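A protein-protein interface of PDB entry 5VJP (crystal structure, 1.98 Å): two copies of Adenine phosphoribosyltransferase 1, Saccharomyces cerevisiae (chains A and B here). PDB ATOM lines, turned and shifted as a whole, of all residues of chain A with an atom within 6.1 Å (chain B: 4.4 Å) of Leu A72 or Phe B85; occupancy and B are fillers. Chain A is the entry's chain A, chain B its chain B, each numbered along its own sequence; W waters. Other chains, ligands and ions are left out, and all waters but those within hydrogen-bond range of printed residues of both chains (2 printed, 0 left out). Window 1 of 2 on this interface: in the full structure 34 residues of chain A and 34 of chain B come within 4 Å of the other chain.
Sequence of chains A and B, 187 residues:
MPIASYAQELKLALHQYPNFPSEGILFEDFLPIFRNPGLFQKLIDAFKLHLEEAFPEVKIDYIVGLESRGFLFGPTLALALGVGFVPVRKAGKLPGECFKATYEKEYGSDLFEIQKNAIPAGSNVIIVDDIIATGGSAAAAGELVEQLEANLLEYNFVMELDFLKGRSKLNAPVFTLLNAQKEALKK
N of Arg A35 sits at hydrogen-bond distance from O of Phe B85, 3.3 Å away. The backbone carbonyl oxygen (O) of Phe A71 lies close to the backbone carbonyl oxygen (O) of Phe B71 (2.9 Å). The backbone NH of Phe B85 lies within hydrogen-bond range of the backbone carbonyl oxygen of Phe A34, 2.7 Å away.
The backbone NH (N) of Ile B63 is in hydrogen-bond range of the backbone carbonyl oxygen (O) of Gly B84 (2.9 Å).
Among the printed residues, pairs that only touch across the chains: Arg A35 with Gly B84 (3.2 Å), Leu A72 with Pro B75 (3.2 Å), Phe A40 with Pro B75 (3.3 Å), Leu A72 with Phe B71 (3.5 Å), Ser A68 with Phe B71 (3.5 Å), Leu A72 with Phe B85 (3.5 Å), Phe A34 with Gly B84 (3.6 Å) and Leu A31 with Pro B87 (3.7 Å).
Printed residues of chain B within 4 Å of Leu A31: Pro B87 (3.7 Å). Of the printed residues of chain B, Leu A72 touches Phe B71 (3.5 Å), Pro B75 (3.2 Å) and Phe B85 (3.5 Å). Of the printed residues of chain A, Phe B71 touches Ser A68, Phe A71 and Leu A72. Gly B74 touches none of the printed residues of chain A. Ala B78 touches none of the printed residues of chain A. Of chain A, only Phe A34 (2.7 Å), Arg A35 (3.3 Å) and Leu A72 (3.5 Å) come within 4 Å of Phe B85. Printed residues of chain A within 4 Å of Pro B87: Leu A31 (3.7 Å). The nearest printed residue of chain B that does not touch Leu A72 is Pro B87 (4.7 Å).
Of the 11 printed residues of chain B, 5 touch a printed residue of chain A. Along chain B the printed residues that touch a printed residue of chain A span positions 71 to 87. Of the 16 printed residues of chain A, 7 touch a printed residue of chain B. Printed residues of chain A that touch a printed residue of chain B: Leu A31, Phe A34, Arg A35, Phe A40, Ser A68, Phe A71 and Leu A72. Hydrophobic or aromatic side chains of chain A within 4 Å of the printed part of chain B: Leu A31, Phe A34, Phe A40, Phe A71 and Leu A72. Among the printed residues, 11 pairs touch across the chains. Among the printed residues, no Asp or Glu carboxylate lies within 4 Å of a Lys or Arg side-chain nitrogen of the other chain.
Phe B71 touches its own counterpart, Phe A71.
Water W1 bridges O of Phe A34 and O of Val B83. Water W2 lies within hydrogen-bond range of the backbone carbonyl oxygen of Phe B85 (2.7 Å) and the backbone carbonyl oxygen of Leu A31 (2.7 Å).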
ATOM      1  N   PHE A  30     -34.294 -19.988   4.418  1.00  0.00           N
ATOM      2  CA  PHE A  30     -34.385 -19.662   5.860  1.00  0.00           C
ATOM      3  C   PHE A  30     -33.371 -18.622   6.377  1.00  0.00           C
ATOM      4  O   PHE A  30     -33.429 -18.237   7.543  1.00  0.00           O
ATOM      5  CB  PHE A  30     -34.409 -20.958   6.714  1.00  0.00           C
ATOM      6  CG  PHE A  30     -33.056 -21.601   6.985  1.00  0.00           C
ATOM      7  CD1 PHE A  30     -31.952 -21.455   6.134  1.00  0.00           C
ATOM      8  CD2 PHE A  30     -32.910 -22.422   8.114  1.00  0.00           C
ATOM      9  CE1 PHE A  30     -30.737 -22.076   6.429  1.00  0.00           C
ATOM     10  CE2 PHE A  30     -31.699 -23.045   8.402  1.00  0.00           C
ATOM     11  CZ  PHE A  30     -30.609 -22.869   7.558  1.00  0.00           C
ATOM     12  N   LEU A  31     -32.492 -18.127   5.506  1.00  0.00           N
ATOM     13  CA  LEU A  31     -31.461 -17.156   5.917  1.00  0.00           C
ATOM     14  C   LEU A  31     -31.971 -15.843   6.515  1.00  0.00           C
ATOM     15  O   LEU A  31     -31.288 -15.276   7.369  1.00  0.00           O
ATOM     16  CB  LEU A  31     -30.476 -16.868   4.779  1.00  0.00           C
ATOM     17  CG  LEU A  31     -29.587 -18.069   4.440  1.00  0.00           C
ATOM     18  CD1 LEU A  31     -28.811 -17.820   3.156  1.00  0.00           C
ATOM     19  CD2 LEU A  31     -28.653 -18.415   5.596  1.00  0.00           C
ATOM     20  N   PHE A  34     -31.846 -15.644  10.328  1.00  0.00           N
ATOM     21  CA  PHE A  34     -30.547 -15.387  10.954  1.00  0.00           C
ATOM     22  C   PHE A  34     -30.136 -13.903  10.978  1.00  0.00           C
ATOM     23  O   PHE A  34     -29.370 -13.506  11.859  1.00  0.00           O
ATOM     24  CB  PHE A  34     -29.450 -16.249  10.311  1.00  0.00           C
ATOM     25  CG  PHE A  34     -29.659 -17.725  10.512  1.00  0.00           C
ATOM     26  CD1 PHE A  34     -29.204 -18.352  11.663  1.00  0.00           C
ATOM     27  CD2 PHE A  34     -30.328 -18.483   9.558  1.00  0.00           C
ATOM     28  CE1 PHE A  34     -29.412 -19.713  11.861  1.00  0.00           C
ATOM     29  CE2 PHE A  34     -30.533 -19.842   9.738  1.00  0.00           C
ATOM     30  CZ  PHE A  34     -30.076 -20.461  10.894  1.00  0.00           C
ATOM     31  N   ARG A  35     -30.634 -13.084  10.041  1.00  0.00           N
ATOM     32  CA  ARG A  35     -30.350 -11.631  10.072  1.00  0.00           C
ATOM     33  C   ARG A  35     -31.091 -10.874  11.164  1.00  0.00           C
ATOM     34  O   ARG A  35     -30.742  -9.741  11.466  1.00  0.00           O
ATOM     35  CB  ARG A  35     -30.621 -10.953   8.731  1.00  0.00           C
ATOM     36  CG  ARG A  35     -32.039 -11.001   8.211  1.00  0.00           C
ATOM     37  CD  ARG A  35     -32.132 -10.388   6.817  1.00  0.00           C
ATOM     38  NE  ARG A  35     -31.533  -9.048   6.740  1.00  0.00           N
ATOM     39  CZ  ARG A  35     -32.191  -7.886   6.733  1.00  0.00           C
ATOM     40  NH1 ARG A  35     -31.498  -6.756   6.655  1.00  0.00           N
ATOM     41  NH2 ARG A  35     -33.521  -7.824   6.790  1.00  0.00           N
ATOM     42  N   ASN A  36     -32.126 -11.480  11.727  1.00  0.00           N
ATOM     43  CA  ASN A  36     -32.931 -10.856  12.769  1.00  0.00           C
ATOM     44  C   ASN A  36     -32.697 -11.637  14.063  1.00  0.00           C
ATOM     45  O   ASN A  36     -33.182 -12.762  14.187  1.00  0.00           O
ATOM     46  CB  ASN A  36     -34.404 -10.890  12.352  1.00  0.00           C
ATOM     47  CG  ASN A  36     -35.297 -10.064  13.257  1.00  0.00           C
ATOM     48  OD1 ASN A  36     -35.246 -10.184  14.479  1.00  0.00           O
ATOM     49  ND2 ASN A  36     -36.142  -9.232  12.653  1.00  0.00           N
ATOM     50  N   PHE A  40     -34.005 -15.297  15.147  1.00  0.00           N
ATOM     51  CA  PHE A  40     -33.006 -16.330  15.375  1.00  0.00           C
ATOM     52  C   PHE A  40     -33.187 -16.945  16.754  1.00  0.00           C
ATOM     53  O   PHE A  40     -33.287 -18.159  16.872  1.00  0.00           O
ATOM     54  CB  PHE A  40     -31.588 -15.776  15.177  1.00  0.00           C
ATOM     55  CG  PHE A  40     -30.487 -16.811  15.292  1.00  0.00           C
ATOM     56  CD1 PHE A  40     -30.716 -18.180  15.062  1.00  0.00           C
ATOM     57  CD2 PHE A  40     -29.199 -16.410  15.608  1.00  0.00           C
ATOM     58  CE1 PHE A  40     -29.693 -19.102  15.181  1.00  0.00           C
ATOM     59  CE2 PHE A  40     -28.174 -17.338  15.712  1.00  0.00           C
ATOM     60  CZ  PHE A  40     -28.418 -18.681  15.499  1.00  0.00           C
ATOM     61  N   ILE A  44     -34.096 -20.956  17.857  1.00  0.00           N
ATOM     62  CA  ILE A  44     -33.329 -21.714  18.840  1.00  0.00           C
ATOM     63  C   ILE A  44     -34.235 -22.130  19.989  1.00  0.00           C
ATOM     64  O   ILE A  44     -34.267 -23.304  20.355  1.00  0.00           O
ATOM     65  CB  ILE A  44     -32.091 -20.927  19.353  1.00  0.00           C
ATOM     66  CG1 ILE A  44     -31.105 -20.663  18.198  1.00  0.00           C
ATOM     67  CG2 ILE A  44     -31.394 -21.664  20.498  1.00  0.00           C
ATOM     68  CD1 ILE A  44     -30.626 -21.891  17.440  1.00  0.00           C
ATOM     69  N   SER A  68     -23.870 -27.951   5.019  1.00  0.00           N
ATOM     70  CA  SER A  68     -23.314 -26.723   5.613  1.00  0.00           C
ATOM     71  C   SER A  68     -24.354 -25.875   6.360  1.00  0.00           C
ATOM     72  O   SER A  68     -23.990 -25.136   7.258  1.00  0.00           O
ATOM     73  CB  SER A  68     -22.602 -25.878   4.542  1.00  0.00           C
ATOM     74  OG  SER A  68     -23.287 -25.909   3.303  1.00  0.00           O
ATOM     75  N   ARG A  69     -25.634 -25.979   5.999  1.00  0.00           N
ATOM     76  CA  ARG A  69     -26.674 -25.124   6.594  1.00  0.00           C
ATOM     77  C   ARG A  69     -27.140 -25.555   7.996  1.00  0.00           C
ATOM     78  O   ARG A  69     -27.673 -24.735   8.751  1.00  0.00           O
ATOM     79  CB  ARG A  69     -27.871 -24.985   5.652  1.00  0.00           C
ATOM     80  CG  ARG A  69     -27.719 -23.858   4.650  1.00  0.00           C
ATOM     81  CD  ARG A  69     -28.904 -23.798   3.702  1.00  0.00           C
ATOM     82  NE  ARG A  69     -28.650 -24.458   2.418  1.00  0.00           N
ATOM     83  CZ  ARG A  69     -29.587 -24.944   1.600  1.00  0.00           C
ATOM     84  NH1 ARG A  69     -30.879 -24.943   1.924  1.00  0.00           N
ATOM     85  NH2 ARG A  69     -29.212 -25.483   0.442  1.00  0.00           N
ATOM     86  N   GLY A  70     -26.939 -26.823   8.349  1.00  0.00           N
ATOM     87  CA  GLY A  70     -27.089 -27.260   9.736  1.00  0.00           C
ATOM     88  C   GLY A  70     -26.137 -26.567  10.696  1.00  0.00           C
ATOM     89  O   GLY A  70     -26.455 -26.405  11.876  1.00  0.00           O
ATOM     90  N   PHE A  71     -24.967 -26.167  10.188  1.00  0.00           N
ATOM     91  CA  PHE A  71     -23.980 -25.374  10.950  1.00  0.00           C
ATOM     92  C   PHE A  71     -24.503 -23.996  11.365  1.00  0.00           C
ATOM     93  O   PHE A  71     -24.001 -23.418  12.330  1.00  0.00           O
ATOM     94  CB  PHE A  71     -22.696 -25.139  10.133  1.00  0.00           C
ATOM     95  CG  PHE A  71     -21.828 -26.357   9.923  1.00  0.00           C
ATOM     96  CD1 PHE A  71     -22.262 -27.661  10.187  1.00  0.00           C
ATOM     97  CD2 PHE A  71     -20.546 -26.183   9.413  1.00  0.00           C
ATOM     98  CE1 PHE A  71     -21.422 -28.741   9.968  1.00  0.00           C
ATOM     99  CE2 PHE A  71     -19.707 -27.265   9.193  1.00  0.00           C
ATOM    100  CZ  PHE A  71     -20.144 -28.545   9.471  1.00  0.00           C
ATOM    101  N   LEU A  72     -25.462 -23.448  10.617  1.00  0.00           N
ATOM    102  CA  LEU A  72     -26.003 -22.118  10.915  1.00  0.00           C
ATOM    103  C   LEU A  72     -26.760 -22.052  12.251  1.00  0.00           C
ATOM    104  O   LEU A  72     -26.682 -21.032  12.943  1.00  0.00           O
ATOM    105  CB  LEU A  72     -26.871 -21.605   9.756  1.00  0.00           C
ATOM    106  CG  LEU A  72     -26.105 -21.335   8.452  1.00  0.00           C
ATOM    107  CD1 LEU A  72     -27.058 -21.179   7.278  1.00  0.00           C
ATOM    108  CD2 LEU A  72     -25.205 -20.107   8.575  1.00  0.00           C
ATOM    109  N   PHE A  73     -27.457 -23.132  12.623  1.00  0.00           N
ATOM    110  CA  PHE A  73     -28.213 -23.171  13.896  1.00  0.00           C
ATOM    111  C   PHE A  73     -27.826 -24.285  14.880  1.00  0.00           C
ATOM    112  O   PHE A  73     -28.054 -24.126  16.079  1.00  0.00           O
ATOM    113  CB  PHE A  73     -29.738 -23.183  13.632  1.00  0.00           C
ATOM    114  CG  PHE A  73     -30.272 -24.502  13.142  1.00  0.00           C
ATOM    115  CD1 PHE A  73     -30.174 -24.857  11.802  1.00  0.00           C
ATOM    116  CD2 PHE A  73     -30.900 -25.379  14.019  1.00  0.00           C
ATOM    117  CE1 PHE A  73     -30.673 -26.074  11.351  1.00  0.00           C
ATOM    118  CE2 PHE A  73     -31.400 -26.591  13.577  1.00  0.00           C
ATOM    119  CZ  PHE A  73     -31.284 -26.943  12.243  1.00  0.00           C
ATOM    120  N   GLY A  74     -27.254 -25.389  14.393  1.00  0.00           N
ATOM    121  CA  GLY A  74     -26.876 -26.526  15.249  1.00  0.00           C
ATOM    122  C   GLY A  74     -25.972 -26.199  16.432  1.00  0.00           C
ATOM    123  O   GLY A  74     -26.306 -26.530  17.574  1.00  0.00           O
ATOM    124  N   PRO A  75     -24.821 -25.546  16.173  1.00  0.00           N
ATOM    125  CA  PRO A  75     -23.929 -25.111  17.242  1.00  0.00           C
ATOM    126  C   PRO A  75     -24.614 -24.180  18.240  1.00  0.00           C
ATOM    127  O   PRO A  75     -24.434 -24.346  19.451  1.00  0.00           O
ATOM    128  CB  PRO A  75     -22.808 -24.379  16.497  1.00  0.00           C
ATOM    129  CG  PRO A  75     -22.810 -24.978  15.137  1.00  0.00           C
ATOM    130  CD  PRO A  75     -24.251 -25.264  14.844  1.00  0.00           C
ATOM    131  N   THR A  76     -25.411 -23.234  17.740  1.00  0.00           N
ATOM    132  CA  THR A  76     -26.122 -22.297  18.615  1.00  0.00           C
ATOM    133  C   THR A  76     -27.160 -23.008  19.481  1.00  0.00           C
ATOM    134  O   THR A  76     -27.319 -22.672  20.655  1.00  0.00           O
ATOM    135  CB  THR A  76     -26.800 -21.161  17.816  1.00  0.00           C
ATOM    136  OG1 THR A  76     -25.860 -20.603  16.892  1.00  0.00           O
ATOM    137  CG2 THR A  76     -27.291 -20.057  18.749  1.00  0.00           C
ATOM    138  N   ILE B  63     -22.837  -9.766  12.002  1.00  0.00           N
ATOM    139  CA  ILE B  63     -21.676 -10.629  11.776  1.00  0.00           C
ATOM    140  C   ILE B  63     -21.856 -11.241  10.388  1.00  0.00           C
ATOM    141  O   ILE B  63     -22.922 -11.775  10.083  1.00  0.00           O
ATOM    142  CB  ILE B  63     -21.573 -11.778  12.799  1.00  0.00           C
ATOM    143  CG1 ILE B  63     -21.548 -11.242  14.238  1.00  0.00           C
ATOM    144  CG2 ILE B  63     -20.353 -12.649  12.511  1.00  0.00           C
ATOM    145  CD1 ILE B  63     -20.422 -10.270  14.547  1.00  0.00           C
ATOM    146  N   GLY B  65     -20.329 -14.239   8.318  1.00  0.00           N
ATOM    147  CA  GLY B  65     -19.511 -15.447   8.448  1.00  0.00           C
ATOM    148  C   GLY B  65     -19.250 -16.137   7.120  1.00  0.00           C
ATOM    149  O   GLY B  65     -20.164 -16.284   6.305  1.00  0.00           O
ATOM    150  N   PHE B  71     -19.405 -20.538   9.840  1.00  0.00           N
ATOM    151  CA  PHE B  71     -20.784 -20.868  10.253  1.00  0.00           C
ATOM    152  C   PHE B  71     -20.856 -21.542  11.629  1.00  0.00           C
ATOM    153  O   PHE B  71     -21.898 -21.485  12.285  1.00  0.00           O
ATOM    154  CB  PHE B  71     -21.457 -21.825   9.248  1.00  0.00           C
ATOM    155  CG  PHE B  71     -21.811 -21.218   7.912  1.00  0.00           C
ATOM    156  CD1 PHE B  71     -21.318 -19.983   7.480  1.00  0.00           C
ATOM    157  CD2 PHE B  71     -22.649 -21.923   7.054  1.00  0.00           C
ATOM    158  CE1 PHE B  71     -21.672 -19.476   6.237  1.00  0.00           C
ATOM    159  CE2 PHE B  71     -22.994 -21.417   5.807  1.00  0.00           C
ATOM    160  CZ  PHE B  71     -22.509 -20.194   5.399  1.00  0.00           C
ATOM    161  N   GLY B  74     -19.885 -18.039  13.975  1.00  0.00           N
ATOM    162  CA  GLY B  74     -20.413 -16.728  13.569  1.00  0.00           C
ATOM    163  C   GLY B  74     -21.848 -16.427  13.979  1.00  0.00           C
ATOM    164  O   GLY B  74     -22.103 -15.396  14.610  1.00  0.00           O
ATOM    165  N   PRO B  75     -22.798 -17.321  13.631  1.00  0.00           N
ATOM    166  CA  PRO B  75     -24.185 -17.167  14.053  1.00  0.00           C
ATOM    167  C   PRO B  75     -24.337 -17.106  15.571  1.00  0.00           C
ATOM    168  O   PRO B  75     -25.084 -16.262  16.074  1.00  0.00           O
ATOM    169  CB  PRO B  75     -24.870 -18.414  13.486  1.00  0.00           C
ATOM    170  CG  PRO B  75     -24.034 -18.812  12.330  1.00  0.00           C
ATOM    171  CD  PRO B  75     -22.629 -18.480  12.739  1.00  0.00           C
ATOM    172  N   ALA B  78     -23.146 -13.793  16.713  1.00  0.00           N
ATOM    173  CA  ALA B  78     -24.214 -12.841  16.346  1.00  0.00           C
ATOM    174  C   ALA B  78     -25.325 -12.798  17.396  1.00  0.00           C
ATOM    175  O   ALA B  78     -25.688 -11.723  17.873  1.00  0.00           O
ATOM    176  CB  ALA B  78     -24.796 -13.165  14.973  1.00  0.00           C
ATOM    177  N   VAL B  83     -27.232  -9.367  17.426  1.00  0.00           N
ATOM    178  CA  VAL B  83     -27.088  -8.816  16.078  1.00  0.00           C
ATOM    179  C   VAL B  83     -27.381  -9.871  15.019  1.00  0.00           C
ATOM    180  O   VAL B  83     -27.462 -11.070  15.307  1.00  0.00           O
ATOM    181  CB  VAL B  83     -25.685  -8.188  15.831  1.00  0.00           C
ATOM    182  CG1 VAL B  83     -25.398  -7.098  16.849  1.00  0.00           C
ATOM    183  CG2 VAL B  83     -24.577  -9.227  15.848  1.00  0.00           C
ATOM    184  N   GLY B  84     -27.550  -9.414  13.789  1.00  0.00           N
ATOM    185  CA  GLY B  84     -27.871 -10.305  12.689  1.00  0.00           C
ATOM    186  C   GLY B  84     -26.667 -11.107  12.241  1.00  0.00           C
ATOM    187  O   GLY B  84     -25.521 -10.700  12.450  1.00  0.00           O
ATOM    188  N   PHE B  85     -26.937 -12.260  11.637  1.00  0.00           N
ATOM    189  CA  PHE B  85     -25.933 -13.034  10.946  1.00  0.00           C
ATOM    190  C   PHE B  85     -26.298 -13.107   9.476  1.00  0.00           C
ATOM    191  O   PHE B  85     -27.468 -13.285   9.132  1.00  0.00           O
ATOM    192  CB  PHE B  85     -25.804 -14.458  11.501  1.00  0.00           C
ATOM    193  CG  PHE B  85     -24.782 -15.273  10.767  1.00  0.00           C
ATOM    194  CD1 PHE B  85     -23.441 -15.204  11.125  1.00  0.00           C
ATOM    195  CD2 PHE B  85     -25.144 -16.046   9.661  1.00  0.00           C
ATOM    196  CE1 PHE B  85     -22.486 -15.919  10.425  1.00  0.00           C
ATOM    197  CE2 PHE B  85     -24.189 -16.758   8.952  1.00  0.00           C
ATOM    198  CZ  PHE B  85     -22.858 -16.700   9.337  1.00  0.00           C
ATOM    199  N   VAL B  86     -25.278 -12.993   8.627  1.00  0.00           N
ATOM    200  CA  VAL B  86     -25.413 -13.144   7.181  1.00  0.00           C
ATOM    201  C   VAL B  86     -24.241 -13.997   6.686  1.00  0.00           C
ATOM    202  O   VAL B  86     -23.096 -13.729   7.030  1.00  0.00           O
ATOM    203  CB  VAL B  86     -25.423 -11.767   6.476  1.00  0.00           C
ATOM    204  CG1 VAL B  86     -25.430 -11.919   4.955  1.00  0.00           C
ATOM    205  CG2 VAL B  86     -26.626 -10.955   6.936  1.00  0.00           C
ATOM    206  N   PRO B  87     -24.520 -15.036   5.882  1.00  0.00           N
ATOM    207  CA  PRO B  87     -23.424 -15.847   5.364  1.00  0.00           C
ATOM    208  C   PRO B  87     -22.806 -15.289   4.085  1.00  0.00           C
ATOM    209  O   PRO B  87     -23.509 -14.700   3.264  1.00  0.00           O
ATOM    210  CB  PRO B  87     -24.105 -17.179   5.069  1.00  0.00           C
ATOM    211  CG  PRO B  87     -25.474 -16.783   4.662  1.00  0.00           C
ATOM    212  CD  PRO B  87     -25.830 -15.597   5.505  1.00  0.00           C
HETATM  213  O   HOH W   1     -29.037 -13.143  14.366  1.00  0.00           O
HETATM  214  O   HOH W   2     -28.713 -14.610   7.187  1.00  0.00           O
